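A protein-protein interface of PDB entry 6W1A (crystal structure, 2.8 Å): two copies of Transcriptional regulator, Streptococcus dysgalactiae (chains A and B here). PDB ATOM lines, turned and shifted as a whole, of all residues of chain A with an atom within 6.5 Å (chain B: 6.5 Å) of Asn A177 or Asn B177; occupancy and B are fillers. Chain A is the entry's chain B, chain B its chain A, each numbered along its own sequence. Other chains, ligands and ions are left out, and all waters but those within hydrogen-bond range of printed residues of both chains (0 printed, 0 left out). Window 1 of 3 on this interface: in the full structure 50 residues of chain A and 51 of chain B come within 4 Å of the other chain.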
ATOM      1  N   ASP A  60     -24.456 -17.715 -25.254  1.00  0.00           N
ATOM      2  CA  ASP A  60     -24.959 -19.082 -25.168  1.00  0.00           C
ATOM      3  C   ASP A  60     -26.482 -19.115 -25.220  1.00  0.00           C
ATOM      4  O   ASP A  60     -27.066 -19.923 -25.951  1.00  0.00           O
ATOM      5  CB  ASP A  60     -24.446 -19.759 -23.896  1.00  0.00           C
ATOM      6  CG  ASP A  60     -24.718 -21.259 -23.879  1.00  0.00           C
ATOM      7  OD1 ASP A  60     -24.211 -21.972 -24.772  1.00  0.00           O
ATOM      8  OD2 ASP A  60     -25.438 -21.725 -22.969  1.00  0.00           O
ATOM      9  N   ALA A 172     -11.216 -27.046 -19.421  1.00  0.00           N
ATOM     10  CA  ALA A 172     -11.789 -25.713 -19.581  1.00  0.00           C
ATOM     11  C   ALA A 172     -12.557 -25.295 -18.331  1.00  0.00           C
ATOM     12  O   ALA A 172     -13.442 -26.012 -17.858  1.00  0.00           O
ATOM     13  CB  ALA A 172     -12.708 -25.673 -20.803  1.00  0.00           C
ATOM     14  N   TYR A 173     -12.244 -24.094 -17.842  1.00  0.00           N
ATOM     15  CA  TYR A 173     -12.622 -23.597 -16.525  1.00  0.00           C
ATOM     16  C   TYR A 173     -13.430 -22.312 -16.656  1.00  0.00           C
ATOM     17  O   TYR A 173     -13.021 -21.398 -17.379  1.00  0.00           O
ATOM     18  CB  TYR A 173     -11.353 -23.268 -15.725  1.00  0.00           C
ATOM     19  CG  TYR A 173     -10.899 -24.231 -14.652  1.00  0.00           C
ATOM     20  CD1 TYR A 173     -11.683 -24.495 -13.538  1.00  0.00           C
ATOM     21  CD2 TYR A 173      -9.646 -24.832 -14.731  1.00  0.00           C
ATOM     22  CE1 TYR A 173     -11.243 -25.356 -12.546  1.00  0.00           C
ATOM     23  CE2 TYR A 173      -9.201 -25.692 -13.751  1.00  0.00           C
ATOM     24  CZ  TYR A 173     -10.001 -25.951 -12.661  1.00  0.00           C
ATOM     25  OH  TYR A 173      -9.554 -26.810 -11.683  1.00  0.00           O
ATOM     26  N   SER A 174     -14.565 -22.237 -15.956  1.00  0.00           N
ATOM     27  CA  SER A 174     -15.274 -20.971 -15.762  1.00  0.00           C
ATOM     28  C   SER A 174     -16.359 -21.157 -14.710  1.00  0.00           C
ATOM     29  O   SER A 174     -16.943 -22.238 -14.597  1.00  0.00           O
ATOM     30  CB  SER A 174     -15.888 -20.450 -17.064  1.00  0.00           C
ATOM     31  OG  SER A 174     -17.177 -20.989 -17.290  1.00  0.00           O
ATOM     32  N   GLU A 175     -16.638 -20.082 -13.959  1.00  0.00           N
ATOM     33  CA  GLU A 175     -17.594 -20.128 -12.855  1.00  0.00           C
ATOM     34  C   GLU A 175     -19.049 -19.939 -13.284  1.00  0.00           C
ATOM     35  O   GLU A 175     -19.948 -20.100 -12.450  1.00  0.00           O
ATOM     36  CB  GLU A 175     -17.201 -19.101 -11.775  1.00  0.00           C
ATOM     37  CG  GLU A 175     -18.108 -19.092 -10.538  1.00  0.00           C
ATOM     38  CD  GLU A 175     -17.739 -20.183  -9.531  1.00  0.00           C
ATOM     39  OE1 GLU A 175     -16.634 -20.766  -9.675  1.00  0.00           O
ATOM     40  OE2 GLU A 175     -18.576 -20.489  -8.636  1.00  0.00           O
ATOM     41  N   GLN A 176     -19.338 -19.700 -14.559  1.00  0.00           N
ATOM     42  CA  GLN A 176     -20.744 -19.657 -14.936  1.00  0.00           C
ATOM     43  C   GLN A 176     -21.247 -20.973 -15.494  1.00  0.00           C
ATOM     44  O   GLN A 176     -22.427 -21.285 -15.327  1.00  0.00           O
ATOM     45  CB  GLN A 176     -21.005 -18.547 -15.960  1.00  0.00           C
ATOM     46  CG  GLN A 176     -22.502 -18.272 -16.237  1.00  0.00           C
ATOM     47  CD  GLN A 176     -23.063 -19.095 -17.399  1.00  0.00           C
ATOM     48  OE1 GLN A 176     -23.747 -20.101 -17.197  1.00  0.00           O
ATOM     49  NE2 GLN A 176     -22.781 -18.658 -18.622  1.00  0.00           N
ATOM     50  N   ASN A 177     -20.375 -21.781 -16.084  1.00  0.00           N
ATOM     51  CA  ASN A 177     -20.752 -23.086 -16.619  1.00  0.00           C
ATOM     52  C   ASN A 177     -19.867 -24.145 -15.973  1.00  0.00           C
ATOM     53  O   ASN A 177     -18.691 -24.276 -16.323  1.00  0.00           O
ATOM     54  CB  ASN A 177     -20.631 -23.113 -18.134  1.00  0.00           C
ATOM     55  CG  ASN A 177     -21.085 -24.426 -18.717  1.00  0.00           C
ATOM     56  OD1 ASN A 177     -22.261 -24.604 -19.016  1.00  0.00           O
ATOM     57  ND2 ASN A 177     -20.154 -25.368 -18.864  1.00  0.00           N
ATOM     58  N   LYS A 178     -20.422 -24.880 -15.013  1.00  0.00           N
ATOM     59  CA  LYS A 178     -19.679 -25.918 -14.316  1.00  0.00           C
ATOM     60  C   LYS A 178     -19.893 -27.303 -14.910  1.00  0.00           C
ATOM     61  O   LYS A 178     -19.473 -28.294 -14.301  1.00  0.00           O
ATOM     62  CB  LYS A 178     -20.070 -25.934 -12.835  1.00  0.00           C
ATOM     63  CG  LYS A 178     -19.867 -24.627 -12.118  1.00  0.00           C
ATOM     64  CD  LYS A 178     -18.428 -24.495 -11.673  1.00  0.00           C
ATOM     65  CE  LYS A 178     -18.226 -23.257 -10.827  1.00  0.00           C
ATOM     66  NZ  LYS A 178     -19.105 -23.266  -9.623  1.00  0.00           N
ATOM     67  N   THR A 179     -20.486 -27.400 -16.101  1.00  0.00           N
ATOM     68  CA  THR A 179     -20.801 -28.721 -16.634  1.00  0.00           C
ATOM     69  C   THR A 179     -19.535 -29.487 -16.997  1.00  0.00           C
ATOM     70  O   THR A 179     -19.459 -30.704 -16.793  1.00  0.00           O
ATOM     71  CB  THR A 179     -21.732 -28.603 -17.843  1.00  0.00           C
ATOM     72  OG1 THR A 179     -20.973 -28.228 -18.998  1.00  0.00           O
ATOM     73  CG2 THR A 179     -22.825 -27.567 -17.597  1.00  0.00           C
ATOM     74  N   ASN A 180     -18.523 -28.793 -17.518  1.00  0.00           N
ATOM     75  CA  ASN A 180     -17.258 -29.458 -17.807  1.00  0.00           C
ATOM     76  C   ASN A 180     -16.557 -29.871 -16.524  1.00  0.00           C
ATOM     77  O   ASN A 180     -16.020 -30.980 -16.434  1.00  0.00           O
ATOM     78  CB  ASN A 180     -16.354 -28.549 -18.638  1.00  0.00           C
ATOM     79  CG  ASN A 180     -16.742 -28.521 -20.095  1.00  0.00           C
ATOM     80  OD1 ASN A 180     -17.690 -29.187 -20.515  1.00  0.00           O
ATOM     81  ND2 ASN A 180     -16.010 -27.745 -20.880  1.00  0.00           N
ATOM     82  N   LYS A 181     -16.563 -28.996 -15.518  1.00  0.00           N
ATOM     83  CA  LYS A 181     -15.923 -29.331 -14.252  1.00  0.00           C
ATOM     84  C   LYS A 181     -16.636 -30.499 -13.581  1.00  0.00           C
ATOM     85  O   LYS A 181     -15.990 -31.390 -13.020  1.00  0.00           O
ATOM     86  CB  LYS A 181     -15.903 -28.103 -13.343  1.00  0.00           C
ATOM     87  CG  LYS A 181     -15.224 -28.317 -12.006  1.00  0.00           C
ATOM     88  CD  LYS A 181     -15.502 -27.164 -11.056  1.00  0.00           C
ATOM     89  CE  LYS A 181     -14.461 -27.119  -9.949  1.00  0.00           C
ATOM     90  NZ  LYS A 181     -14.708 -26.008  -8.988  1.00  0.00           N
ATOM     91  N   ASP B  60     -19.742 -21.677 -25.895  1.00  0.00           N
ATOM     92  CA  ASP B  60     -19.583 -21.311 -24.490  1.00  0.00           C
ATOM     93  C   ASP B  60     -18.138 -21.484 -24.031  1.00  0.00           C
ATOM     94  O   ASP B  60     -17.594 -20.606 -23.351  1.00  0.00           O
ATOM     95  CB  ASP B  60     -20.526 -22.128 -23.607  1.00  0.00           C
ATOM     96  CG  ASP B  60     -20.618 -21.574 -22.186  1.00  0.00           C
ATOM     97  OD1 ASP B  60     -20.182 -22.261 -21.235  1.00  0.00           O
ATOM     98  OD2 ASP B  60     -21.121 -20.444 -22.019  1.00  0.00           O
ATOM     99  N   GLU B  61     -17.497 -22.603 -24.387  1.00  0.00           N
ATOM    100  CA  GLU B  61     -16.090 -22.779 -24.038  1.00  0.00           C
ATOM    101  C   GLU B  61     -15.213 -21.734 -24.711  1.00  0.00           C
ATOM    102  O   GLU B  61     -14.248 -21.247 -24.112  1.00  0.00           O
ATOM    103  CB  GLU B  61     -15.603 -24.172 -24.435  1.00  0.00           C
ATOM    104  CG  GLU B  61     -16.145 -25.322 -23.629  1.00  0.00           C
ATOM    105  CD  GLU B  61     -15.716 -26.653 -24.206  1.00  0.00           C
ATOM    106  OE1 GLU B  61     -15.149 -26.666 -25.315  1.00  0.00           O
ATOM    107  OE2 GLU B  61     -15.957 -27.688 -23.562  1.00  0.00           O
ATOM    108  N   SER B  64     -15.279 -18.363 -23.061  1.00  0.00           N
ATOM    109  CA  SER B  64     -14.725 -18.535 -21.724  1.00  0.00           C
ATOM    110  C   SER B  64     -13.363 -19.215 -21.791  1.00  0.00           C
ATOM    111  O   SER B  64     -13.010 -19.994 -20.900  1.00  0.00           O
ATOM    112  CB  SER B  64     -15.681 -19.284 -20.796  1.00  0.00           C
ATOM    113  OG  SER B  64     -15.373 -20.654 -20.714  1.00  0.00           O
ATOM    114  N   ALA B 172     -35.090 -19.347 -20.488  1.00  0.00           N
ATOM    115  CA  ALA B 172     -34.406 -20.038 -21.575  1.00  0.00           C
ATOM    116  C   ALA B 172     -33.312 -20.949 -21.029  1.00  0.00           C
ATOM    117  O   ALA B 172     -32.392 -20.476 -20.353  1.00  0.00           O
ATOM    118  CB  ALA B 172     -33.813 -19.034 -22.562  1.00  0.00           C
ATOM    119  N   TYR B 173     -33.404 -22.245 -21.322  1.00  0.00           N
ATOM    120  CA  TYR B 173     -32.413 -23.209 -20.857  1.00  0.00           C
ATOM    121  C   TYR B 173     -32.005 -24.098 -22.025  1.00  0.00           C
ATOM    122  O   TYR B 173     -32.862 -24.604 -22.759  1.00  0.00           O
ATOM    123  CB  TYR B 173     -32.915 -24.013 -19.649  1.00  0.00           C
ATOM    124  CG  TYR B 173     -33.575 -25.343 -19.918  1.00  0.00           C
ATOM    125  CD1 TYR B 173     -32.880 -26.531 -19.741  1.00  0.00           C
ATOM    126  CD2 TYR B 173     -34.910 -25.412 -20.298  1.00  0.00           C
ATOM    127  CE1 TYR B 173     -33.487 -27.751 -19.962  1.00  0.00           C
ATOM    128  CE2 TYR B 173     -35.526 -26.627 -20.522  1.00  0.00           C
ATOM    129  CZ  TYR B 173     -34.810 -27.793 -20.352  1.00  0.00           C
ATOM    130  OH  TYR B 173     -35.416 -29.005 -20.574  1.00  0.00           O
ATOM    131  N   SER B 174     -30.699 -24.254 -22.209  1.00  0.00           N
ATOM    132  CA  SER B 174     -30.153 -25.220 -23.150  1.00  0.00           C
ATOM    133  C   SER B 174     -30.010 -26.595 -22.509  1.00  0.00           C
ATOM    134  O   SER B 174     -29.815 -26.722 -21.297  1.00  0.00           O
ATOM    135  CB  SER B 174     -28.790 -24.744 -23.659  1.00  0.00           C
ATOM    136  OG  SER B 174     -27.998 -25.833 -24.092  1.00  0.00           O
ATOM    137  N   GLU B 175     -30.114 -27.633 -23.342  1.00  0.00           N
ATOM    138  CA  GLU B 175     -29.989 -28.999 -22.848  1.00  0.00           C
ATOM    139  C   GLU B 175     -28.534 -29.413 -22.685  1.00  0.00           C
ATOM    140  O   GLU B 175     -28.259 -30.458 -22.085  1.00  0.00           O
ATOM    141  CB  GLU B 175     -30.719 -29.954 -23.806  1.00  0.00           C
ATOM    142  CG  GLU B 175     -30.677 -31.442 -23.449  1.00  0.00           C
ATOM    143  CD  GLU B 175     -31.635 -31.820 -22.335  1.00  0.00           C
ATOM    144  OE1 GLU B 175     -32.625 -31.089 -22.115  1.00  0.00           O
ATOM    145  OE2 GLU B 175     -31.397 -32.857 -21.680  1.00  0.00           O
ATOM    146  N   GLN B 176     -27.596 -28.582 -23.135  1.00  0.00           N
ATOM    147  CA  GLN B 176     -26.181 -28.800 -22.873  1.00  0.00           C
ATOM    148  C   GLN B 176     -25.650 -27.932 -21.745  1.00  0.00           C
ATOM    149  O   GLN B 176     -24.668 -28.305 -21.096  1.00  0.00           O
ATOM    150  CB  GLN B 176     -25.357 -28.538 -24.136  1.00  0.00           C
ATOM    151  CG  GLN B 176     -23.950 -29.090 -24.042  1.00  0.00           C
ATOM    152  CD  GLN B 176     -23.176 -28.957 -25.331  1.00  0.00           C
ATOM    153  OE1 GLN B 176     -21.952 -28.856 -25.317  1.00  0.00           O
ATOM    154  NE2 GLN B 176     -23.883 -28.945 -26.457  1.00  0.00           N
ATOM    155  N   ASN B 177     -26.275 -26.782 -21.501  1.00  0.00           N
ATOM    156  CA  ASN B 177     -25.909 -25.875 -20.417  1.00  0.00           C
ATOM    157  C   ASN B 177     -27.161 -25.675 -19.571  1.00  0.00           C
ATOM    158  O   ASN B 177     -28.030 -24.868 -19.911  1.00  0.00           O
ATOM    159  CB  ASN B 177     -25.376 -24.555 -20.964  1.00  0.00           C
ATOM    160  CG  ASN B 177     -24.910 -23.613 -19.875  1.00  0.00           C
ATOM    161  OD1 ASN B 177     -25.133 -23.850 -18.690  1.00  0.00           O
ATOM    162  ND2 ASN B 177     -24.245 -22.536 -20.276  1.00  0.00           N
ATOM    163  N   LYS B 178     -27.235 -26.393 -18.457  1.00  0.00           N
ATOM    164  CA  LYS B 178     -28.386 -26.358 -17.570  1.00  0.00           C
ATOM    165  C   LYS B 178     -28.213 -25.368 -16.427  1.00  0.00           C
ATOM    166  O   LYS B 178     -28.889 -25.497 -15.401  1.00  0.00           O
ATOM    167  CB  LYS B 178     -28.679 -27.758 -17.035  1.00  0.00           C
ATOM    168  CG  LYS B 178     -28.842 -28.796 -18.134  1.00  0.00           C
ATOM    169  CD  LYS B 178     -29.827 -29.878 -17.739  1.00  0.00           C
ATOM    170  CE  LYS B 178     -29.596 -31.154 -18.529  1.00  0.00           C
ATOM    171  NZ  LYS B 178     -28.321 -31.829 -18.128  1.00  0.00           N
ATOM    172  N   THR B 179     -27.315 -24.391 -16.577  1.00  0.00           N
ATOM    173  CA  THR B 179     -27.029 -23.475 -15.478  1.00  0.00           C
ATOM    174  C   THR B 179     -28.246 -22.620 -15.137  1.00  0.00           C
ATOM    175  O   THR B 179     -28.544 -22.393 -13.956  1.00  0.00           O
ATOM    176  CB  THR B 179     -25.842 -22.583 -15.852  1.00  0.00           C
ATOM    177  OG1 THR B 179     -24.642 -23.365 -15.879  1.00  0.00           O
ATOM    178  CG2 THR B 179     -25.682 -21.426 -14.864  1.00  0.00           C
ATOM    179  N   ASN B 180     -28.994 -22.181 -16.154  1.00  0.00           N
ATOM    180  CA  ASN B 180     -30.208 -21.416 -15.892  1.00  0.00           C
ATOM    181  C   ASN B 180     -31.282 -22.286 -15.257  1.00  0.00           C
ATOM    182  O   ASN B 180     -31.975 -21.848 -14.330  1.00  0.00           O
ATOM    183  CB  ASN B 180     -30.729 -20.789 -17.183  1.00  0.00           C
ATOM    184  CG  ASN B 180     -29.904 -19.602 -17.623  1.00  0.00           C
ATOM    185  OD1 ASN B 180     -28.954 -19.211 -16.949  1.00  0.00           O
ATOM    186  ND2 ASN B 180     -30.257 -19.027 -18.765  1.00  0.00           N
ATOM    187  N   LYS B 181     -31.433 -23.521 -15.739  1.00  0.00           N
ATOM    188  CA  LYS B 181     -32.461 -24.393 -15.187  1.00  0.00           C
ATOM    189  C   LYS B 181     -32.175 -24.724 -13.734  1.00  0.00           C
ATOM    190  O   LYS B 181     -33.088 -24.714 -12.905  1.00  0.00           O
ATOM    191  CB  LYS B 181     -32.574 -25.672 -16.012  1.00  0.00           C
ATOM    192  CG  LYS B 181     -33.658 -26.622 -15.535  1.00  0.00           C
ATOM    193  CD  LYS B 181     -33.491 -27.992 -16.181  1.00  0.00           C
ATOM    194  CE  LYS B 181     -34.786 -28.791 -16.143  1.00  0.00           C
ATOM    195  NZ  LYS B 181     -34.623 -30.137 -16.764  1.00  0.00           N
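The side-chain amide nitrogen (ND2) of Asn A180 is in hydrogen-bond range of the side-chain carboxylate (OE2) of Glu B61, at 2.7 Å. The side-chain carboxylate (OD2) of Asp A60 lies within hydrogen-bond range of the side-chain amide nitrogen (ND2) of Asn B177 (3.1 Å). The side-chain amide oxygen (OD1) of Asn A177 sits close to the side-chain amide oxygen (OD1) of Asn B177, at 3.0 Å. OG1 of Thr B179 is in hydrogen-bond range of O of Gln A176, 3.1 Å away.
Of the 11 printed residues of chain A, 6 touch a printed residue of chain B. Of the 13 printed residues of chain B, 5 touch a printed residue of chain A. Printed residues of chain B that touch a printed residue of chain A: Asp B60, Glu B61, Ser B64, Asn B177 and Thr B179. Among the printed residues, 10 pairs touch across the chains. Among the printed residues, no Asp or Glu carboxylate lies within 4 Å of a Lys or Arg side-chain nitrogen of the other chain.
Asp B60 touches its own counterpart, Asp A60. Asp A60 touches Asn B177, and with the chains exchanged Asn A177 touches Asp B60. Gln A176 touches Asn B177, but with the chains exchanged Asn A177 does not touch Gln B176 (4.9 Å). Asn A177 touches Thr B179, but with the chains exchanged Thr A179 does not touch Asn B177 (4.5 Å). Positions printed for both chains: 60, 172, 173, 174, 175, 176, 177, 178, 179, 180 and 181. Of the 10 pairs that touch across the chains among the printed residues, 4 have their exchanged pair printed and touching as well.
Of the printed residues of chain B, Asp A60 touches Asp B60 and Asn B177. Of the printed residues of chain B, Gln A176 touches Asn B177 (3.96 Å) and Thr B179 (3.1 Å). Asn A177 touches just these residues of chain B: Asp B60, Asn B177 and Thr B179. Thr A179 touches none of the printed residues of chain B. Of the printed residues of chain A, Asp B60 touches Asp A60 (3.9 Å) and Asn A177 (3.2 Å). Glu B175 touches none of the printed residues of chain A. Asn B177 touches just these residues of chain A: Asp A60 (3.1 Å), Gln A176 (3.96 Å) and Asn A177 (3.0 Å). Printed residues of chain A within 4 Å of Thr B179: Gln A176 and Asn A177.
Asp A60 touches Asp B60 (OD1 to CB, 3.9 Å). O of Tyr A173 touches O of Ser B64 (3.8 Å). Ser A174 touches Ser B64 (CB to OG, 3.7 Å). Gln A176 touches Asn B177. Asp B60 touches Asn A177. Thr B179 touches Asn A177 (OG1 to CA, 3.97 Å).
The backbone carbonyl oxygen (O) of Asp B60 is in hydrogen-bond range of the side-chain hydroxyl (OG) of Ser B64 (3.4 Å). The side-chain hydroxyl (OG) of Ser B174 sits at hydrogen-bond distance from the backbone NH (N) of Asn B177 (3.3 Å). The side-chain amide oxygen (OD1) of Asn B177 sits at hydrogen-bond distance from the side-chain hydroxyl (OG1) of Thr B179 (2.9 Å). The side-chain amide nitrogen (ND2) of Asn A177 is in hydrogen-bond range of the side-chain hydroxyl (OG1) of Thr A179.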
